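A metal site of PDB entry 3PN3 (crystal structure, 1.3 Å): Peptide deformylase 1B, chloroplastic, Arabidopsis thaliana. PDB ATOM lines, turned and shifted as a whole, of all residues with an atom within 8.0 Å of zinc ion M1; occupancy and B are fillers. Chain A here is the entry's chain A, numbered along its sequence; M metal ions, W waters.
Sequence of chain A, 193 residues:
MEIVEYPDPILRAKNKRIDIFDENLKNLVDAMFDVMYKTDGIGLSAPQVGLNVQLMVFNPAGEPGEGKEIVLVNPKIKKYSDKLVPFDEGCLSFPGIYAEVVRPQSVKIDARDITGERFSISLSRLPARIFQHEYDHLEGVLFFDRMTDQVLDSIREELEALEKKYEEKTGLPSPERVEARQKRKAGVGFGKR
Gln 48 touches zinc ion M1 (NE2 to ZN, 3.3 Å). The nearest printed residue that does not touch zinc ion M1 is Glu 134 (4.1 Å).
OE2 of Glu 89 lies within hydrogen-bond range of ND1 of His 133. A ring nitrogen (NE2) of His 137 lies close to the side-chain amide nitrogen of Gln 48. SG of Cys 91 sits close to N of Ser 93, 3.5 Å away. The side-chain hydroxyl (OG) of Ser 93 sits at hydrogen-bond distance from the side-chain amide nitrogen (NE2) of Gln 48, at 2.9 Å. OG of Ser 45 lies close to OE1 of Gln 48 (3.4 Å). O of Gln 48 is in hydrogen-bond range of N of Val 4 (2.8 Å).
Zinc ion M1 is bound by water W1 (2.0 Å), a ring nitrogen (NE2) of His 133 (2.0 Å), a ring nitrogen (NE2) of His 137 (2.1 Å) and the side-chain sulfur of Cys 91 (2.3 Å). Zinc ion M1 has four donor atoms within binding distance.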
ATOM      1  N   ILE A   3      24.466 -30.968  16.045  1.00  0.00           N
ATOM      2  CA  ILE A   3      24.730 -29.935  15.048  1.00  0.00           C
ATOM      3  C   ILE A   3      24.092 -30.405  13.754  1.00  0.00           C
ATOM      4  O   ILE A   3      24.398 -31.491  13.245  1.00  0.00           O
ATOM      5  CB  ILE A   3      26.240 -29.658  14.881  1.00  0.00           C
ATOM      6  CG1 ILE A   3      26.823 -28.982  16.145  1.00  0.00           C
ATOM      7  CG2 ILE A   3      26.505 -28.823  13.612  1.00  0.00           C
ATOM      8  CD1 ILE A   3      26.320 -27.563  16.420  1.00  0.00           C
ATOM      9  N   VAL A   4      23.191 -29.584  13.239  1.00  0.00           N
ATOM     10  CA  VAL A   4      22.494 -29.843  11.980  1.00  0.00           C
ATOM     11  C   VAL A   4      23.476 -29.656  10.820  1.00  0.00           C
ATOM     12  O   VAL A   4      24.187 -28.657  10.772  1.00  0.00           O
ATOM     13  CB  VAL A   4      21.289 -28.875  11.838  1.00  0.00           C
ATOM     14  CG1 VAL A   4      20.647 -28.995  10.468  1.00  0.00           C
ATOM     15  CG2 VAL A   4      20.263 -29.157  12.925  1.00  0.00           C
ATOM     16  N   LEU A  11      18.764 -25.316   7.970  1.00  0.00           N
ATOM     17  CA  LEU A  11      19.813 -24.318   7.773  1.00  0.00           C
ATOM     18  C   LEU A  11      19.467 -23.223   6.767  1.00  0.00           C
ATOM     19  O   LEU A  11      20.208 -22.254   6.631  1.00  0.00           O
ATOM     20  CB  LEU A  11      21.127 -24.990   7.376  1.00  0.00           C
ATOM     21  CG  LEU A  11      21.693 -25.993   8.379  1.00  0.00           C
ATOM     22  CD1 LEU A  11      22.870 -26.719   7.781  1.00  0.00           C
ATOM     23  CD2 LEU A  11      22.082 -25.336   9.711  1.00  0.00           C
ATOM     24  N   GLY A  43      31.213 -18.713  18.424  1.00  0.00           N
ATOM     25  CA  GLY A  43      29.803 -18.366  18.330  1.00  0.00           C
ATOM     26  C   GLY A  43      28.981 -19.539  17.852  1.00  0.00           C
ATOM     27  O   GLY A  43      29.513 -20.420  17.182  1.00  0.00           O
ATOM     28  N   LEU A  44      27.705 -19.549  18.201  1.00  0.00           N
ATOM     29  CA  LEU A  44      26.790 -20.599  17.763  1.00  0.00           C
ATOM     30  C   LEU A  44      25.403 -20.017  17.565  1.00  0.00           C
ATOM     31  O   LEU A  44      24.875 -19.330  18.439  1.00  0.00           O
ATOM     32  CB  LEU A  44      26.737 -21.756  18.769  1.00  0.00           C
ATOM     33  CG  LEU A  44      25.744 -22.889  18.474  1.00  0.00           C
ATOM     34  CD1 LEU A  44      26.042 -23.625  17.173  1.00  0.00           C
ATOM     35  CD2 LEU A  44      25.725 -23.876  19.628  1.00  0.00           C
ATOM     36  N   SER A  45      24.827 -20.321  16.403  1.00  0.00           N
ATOM     37  CA  SER A  45      23.501 -19.850  16.019  1.00  0.00           C
ATOM     38  C   SER A  45      22.458 -20.951  16.239  1.00  0.00           C
ATOM     39  O   SER A  45      22.747 -22.128  16.031  1.00  0.00           O
ATOM     40  CB  SER A  45      23.512 -19.447  14.554  1.00  0.00           C
ATOM     41  OG  SER A  45      23.938 -20.534  13.746  1.00  0.00           O
ATOM     42  N   GLN A  48      21.688 -23.998  13.833  1.00  0.00           N
ATOM     43  CA  GLN A  48      22.656 -25.093  13.835  1.00  0.00           C
ATOM     44  C   GLN A  48      22.409 -26.157  14.894  1.00  0.00           C
ATOM     45  O   GLN A  48      22.934 -27.266  14.774  1.00  0.00           O
ATOM     46  CB  GLN A  48      24.075 -24.554  13.956  1.00  0.00           C
ATOM     47  CG  GLN A  48      24.587 -23.968  12.674  1.00  0.00           C
ATOM     48  CD  GLN A  48      26.056 -23.712  12.749  1.00  0.00           C
ATOM     49  OE1 GLN A  48      26.488 -22.753  13.391  1.00  0.00           O
ATOM     50  NE2 GLN A  48      26.838 -24.570  12.114  1.00  0.00           N
ATOM     51  N   GLU A  89      37.906 -20.457   6.148  1.00  0.00           N
ATOM     52  CA  GLU A  89      36.750 -20.577   7.010  1.00  0.00           C
ATOM     53  C   GLU A  89      36.235 -22.009   7.054  1.00  0.00           C
ATOM     54  O   GLU A  89      36.295 -22.734   6.059  1.00  0.00           O
ATOM     55  CB  GLU A  89      35.661 -19.647   6.476  1.00  0.00           C
ATOM     56  CG  GLU A  89      34.659 -19.157   7.498  1.00  0.00           C
ATOM     57  CD  GLU A  89      33.738 -18.101   6.910  1.00  0.00           C
ATOM     58  OE1 GLU A  89      34.195 -16.971   6.614  1.00  0.00           O
ATOM     59  OE2 GLU A  89      32.548 -18.412   6.743  1.00  0.00           O
ATOM     60  N   GLY A  90      35.724 -22.404   8.216  1.00  0.00           N
ATOM     61  CA  GLY A  90      35.057 -23.687   8.376  1.00  0.00           C
ATOM     62  C   GLY A  90      33.636 -23.498   8.857  1.00  0.00           C
ATOM     63  O   GLY A  90      33.178 -22.372   9.066  1.00  0.00           O
ATOM     64  N   CYS A  91      32.933 -24.615   9.034  1.00  0.00           N
ATOM     65  CA  CYS A  91      31.544 -24.611   9.476  1.00  0.00           C
ATOM     66  C   CYS A  91      31.181 -25.982  10.017  1.00  0.00           C
ATOM     67  O   CYS A  91      31.329 -26.974   9.323  1.00  0.00           O
ATOM     68  CB  CYS A  91      30.603 -24.268   8.310  1.00  0.00           C
ATOM     69  SG  CYS A  91      28.836 -24.243   8.763  1.00  0.00           S
ATOM     70  N   LEU A  92      30.691 -26.042  11.258  1.00  0.00           N
ATOM     71  CA  LEU A  92      30.314 -27.318  11.861  1.00  0.00           C
ATOM     72  C   LEU A  92      29.238 -28.071  11.078  1.00  0.00           C
ATOM     73  O   LEU A  92      29.111 -29.283  11.200  1.00  0.00           O
ATOM     74  CB  LEU A  92      29.881 -27.125  13.315  1.00  0.00           C
ATOM     75  CG  LEU A  92      30.941 -26.683  14.326  1.00  0.00           C
ATOM     76  CD1 LEU A  92      30.308 -26.563  15.698  1.00  0.00           C
ATOM     77  CD2 LEU A  92      32.123 -27.639  14.356  1.00  0.00           C
ATOM     78  N   SER A  93      28.445 -27.336  10.289  1.00  0.00           N
ATOM     79  CA  SER A  93      27.421 -27.955   9.459  1.00  0.00           C
ATOM     80  C   SER A  93      27.989 -28.623   8.194  1.00  0.00           C
ATOM     81  O   SER A  93      27.257 -29.306   7.471  1.00  0.00           O
ATOM     82  CB  SER A  93      26.352 -26.928   9.085  1.00  0.00           C
ATOM     83  OG  SER A  93      25.682 -26.478  10.254  1.00  0.00           O
ATOM     84  N   PHE A  94      29.276 -28.412   7.939  1.00  0.00           N
ATOM     85  CA  PHE A  94      29.982 -29.011   6.810  1.00  0.00           C
ATOM     86  C   PHE A  94      31.261 -29.642   7.360  1.00  0.00           C
ATOM     87  O   PHE A  94      32.346 -29.097   7.189  1.00  0.00           O
ATOM     88  CB  PHE A  94      30.373 -27.932   5.785  1.00  0.00           C
ATOM     89  CG  PHE A  94      29.209 -27.204   5.155  1.00  0.00           C
ATOM     90  CD1 PHE A  94      28.538 -26.195   5.839  1.00  0.00           C
ATOM     91  CD2 PHE A  94      28.843 -27.479   3.832  1.00  0.00           C
ATOM     92  CE1 PHE A  94      27.489 -25.498   5.236  1.00  0.00           C
ATOM     93  CE2 PHE A  94      27.807 -26.779   3.227  1.00  0.00           C
ATOM     94  CZ  PHE A  94      27.128 -25.794   3.925  1.00  0.00           C
ATOM     95  N   ARG A 103      35.461 -11.602   3.578  1.00  0.00           N
ATOM     96  CA  ARG A 103      34.435 -10.867   4.322  1.00  0.00           C
ATOM     97  C   ARG A 103      34.992  -9.541   4.831  1.00  0.00           C
ATOM     98  O   ARG A 103      36.205  -9.397   4.967  1.00  0.00           O
ATOM     99  CB  ARG A 103      33.970 -11.645   5.549  1.00  0.00           C
ATOM    100  CG  ARG A 103      33.178 -12.916   5.292  1.00  0.00           C
ATOM    101  CD  ARG A 103      32.708 -13.486   6.614  1.00  0.00           C
ATOM    102  NE  ARG A 103      32.245 -14.867   6.473  1.00  0.00           N
ATOM    103  CZ  ARG A 103      30.994 -15.225   6.216  1.00  0.00           C
ATOM    104  NH1 ARG A 103      30.038 -14.313   6.077  1.00  0.00           N
ATOM    105  NH2 ARG A 103      30.704 -16.514   6.110  1.00  0.00           N
ATOM    106  N   ILE A 130      33.846 -14.678  12.871  1.00  0.00           N
ATOM    107  CA  ILE A 130      32.932 -15.691  13.385  1.00  0.00           C
ATOM    108  C   ILE A 130      31.522 -15.131  13.485  1.00  0.00           C
ATOM    109  O   ILE A 130      30.545 -15.789  13.119  1.00  0.00           O
ATOM    110  CB  ILE A 130      33.406 -16.253  14.740  1.00  0.00           C
ATOM    111  CG1 ILE A 130      34.785 -16.919  14.615  1.00  0.00           C
ATOM    112  CG2 ILE A 130      32.358 -17.223  15.321  1.00  0.00           C
ATOM    113  CD1 ILE A 130      34.875 -18.077  13.620  1.00  0.00           C
ATOM    114  N   HIS A 133      29.891 -15.102  10.085  1.00  0.00           N
ATOM    115  CA  HIS A 133      29.565 -16.465   9.716  1.00  0.00           C
ATOM    116  C   HIS A 133      28.273 -16.946  10.406  1.00  0.00           C
ATOM    117  O   HIS A 133      27.376 -17.501   9.756  1.00  0.00           O
ATOM    118  CB  HIS A 133      30.733 -17.379  10.040  1.00  0.00           C
ATOM    119  CG  HIS A 133      30.453 -18.819   9.750  1.00  0.00           C
ATOM    120  ND1 HIS A 133      30.897 -19.444   8.600  1.00  0.00           N
ATOM    121  CD2 HIS A 133      29.749 -19.742  10.439  1.00  0.00           C
ATOM    122  CE1 HIS A 133      30.477 -20.703   8.604  1.00  0.00           C
ATOM    123  NE2 HIS A 133      29.776 -20.906   9.709  1.00  0.00           N
ATOM    124  N   GLU A 134      28.177 -16.713  11.707  1.00  0.00           N
ATOM    125  CA  GLU A 134      26.996 -17.107  12.472  1.00  0.00           C
ATOM    126  C   GLU A 134      25.762 -16.267  12.156  1.00  0.00           C
ATOM    127  O   GLU A 134      24.649 -16.778  12.174  1.00  0.00           O
ATOM    128  CB  GLU A 134      27.305 -17.096  13.971  1.00  0.00           C
ATOM    129  CG  GLU A 134      28.385 -18.092  14.375  1.00  0.00           C
ATOM    130  CD  GLU A 134      27.971 -19.538  14.099  1.00  0.00           C
ATOM    131  OE1 GLU A 134      26.784 -19.870  14.308  1.00  0.00           O
ATOM    132  OE2 GLU A 134      28.831 -20.332  13.668  1.00  0.00           O
ATOM    133  N   ASP A 136      25.143 -14.967   9.205  1.00  0.00           N
ATOM    134  CA  ASP A 136      24.671 -15.573   7.973  1.00  0.00           C
ATOM    135  C   ASP A 136      23.758 -16.767   8.273  1.00  0.00           C
ATOM    136  O   ASP A 136      22.698 -16.896   7.667  1.00  0.00           O
ATOM    137  CB  ASP A 136      25.838 -16.020   7.091  1.00  0.00           C
ATOM    138  CG  ASP A 136      26.425 -14.896   6.248  1.00  0.00           C
ATOM    139  OD1 ASP A 136      27.391 -15.185   5.522  1.00  0.00           O
ATOM    140  OD2 ASP A 136      25.931 -13.746   6.283  1.00  0.00           O
ATOM    141  N   HIS A 137      24.136 -17.628   9.223  1.00  0.00           N
ATOM    142  CA  HIS A 137      23.272 -18.756   9.594  1.00  0.00           C
ATOM    143  C   HIS A 137      21.871 -18.273   9.995  1.00  0.00           C
ATOM    144  O   HIS A 137      20.880 -18.925   9.658  1.00  0.00           O
ATOM    145  CB  HIS A 137      23.852 -19.552  10.762  1.00  0.00           C
ATOM    146  CG  HIS A 137      24.865 -20.575  10.360  1.00  0.00           C
ATOM    147  ND1 HIS A 137      24.568 -21.651   9.541  1.00  0.00           N
ATOM    148  CD2 HIS A 137      26.174 -20.731  10.717  1.00  0.00           C
ATOM    149  CE1 HIS A 137      25.648 -22.390   9.382  1.00  0.00           C
ATOM    150  NE2 HIS A 137      26.633 -21.863  10.090  1.00  0.00           N
ATOM    151  N   VAL A 141      21.858 -18.248   5.316  1.00  0.00           N
ATOM    152  CA  VAL A 141      22.967 -18.132   4.372  1.00  0.00           C
ATOM    153  C   VAL A 141      24.121 -18.998   4.870  1.00  0.00           C
ATOM    154  O   VAL A 141      24.480 -18.959   6.040  1.00  0.00           O
ATOM    155  CB  VAL A 141      23.393 -16.648   4.194  1.00  0.00           C
ATOM    156  CG1 VAL A 141      24.681 -16.528   3.396  1.00  0.00           C
ATOM    157  CG2 VAL A 141      22.277 -15.847   3.529  1.00  0.00           C
ATOM    158  N   LEU A 142      24.682 -19.799   3.960  1.00  0.00           N
ATOM    159  CA  LEU A 142      25.742 -20.744   4.304  1.00  0.00           C
ATOM    160  C   LEU A 142      27.048 -20.332   3.624  1.00  0.00           C
ATOM    161  O   LEU A 142      27.021 -19.637   2.608  1.00  0.00           O
ATOM    162  CB  LEU A 142      25.331 -22.162   3.916  1.00  0.00           C
ATOM    163  CG  LEU A 142      24.046 -22.642   4.599  1.00  0.00           C
ATOM    164  CD1 LEU A 142      23.684 -24.068   4.158  1.00  0.00           C
ATOM    165  CD2 LEU A 142      24.158 -22.567   6.127  1.00  0.00           C
ATOM    166  N   PHE A 143      28.173 -20.758   4.178  1.00  0.00           N
ATOM    167  CA  PHE A 143      29.450 -20.137   3.829  1.00  0.00           C
ATOM    168  C   PHE A 143      29.895 -20.317   2.374  1.00  0.00           C
ATOM    169  O   PHE A 143      30.601 -19.473   1.830  1.00  0.00           O
ATOM    170  CB  PHE A 143      30.560 -20.420   4.860  1.00  0.00           C
ATOM    171  CG  PHE A 143      31.184 -21.809   4.792  1.00  0.00           C
ATOM    172  CD1 PHE A 143      32.538 -21.953   5.083  1.00  0.00           C
ATOM    173  CD2 PHE A 143      30.450 -22.944   4.480  1.00  0.00           C
ATOM    174  CE1 PHE A 143      33.157 -23.192   5.057  1.00  0.00           C
ATOM    175  CE2 PHE A 143      31.066 -24.204   4.447  1.00  0.00           C
ATOM    176  CZ  PHE A 143      32.430 -24.326   4.738  1.00  0.00           C
HETATM  177 ZN    ZN M   1      28.622 -22.491  10.198  1.00  0.00          ZN
HETATM  178 ZN    ZN M   2      28.348 -22.206  13.711  1.00  0.00          ZN
HETATM  179  O   HOH W   1      29.079 -22.892  12.058  1.00  0.00           O
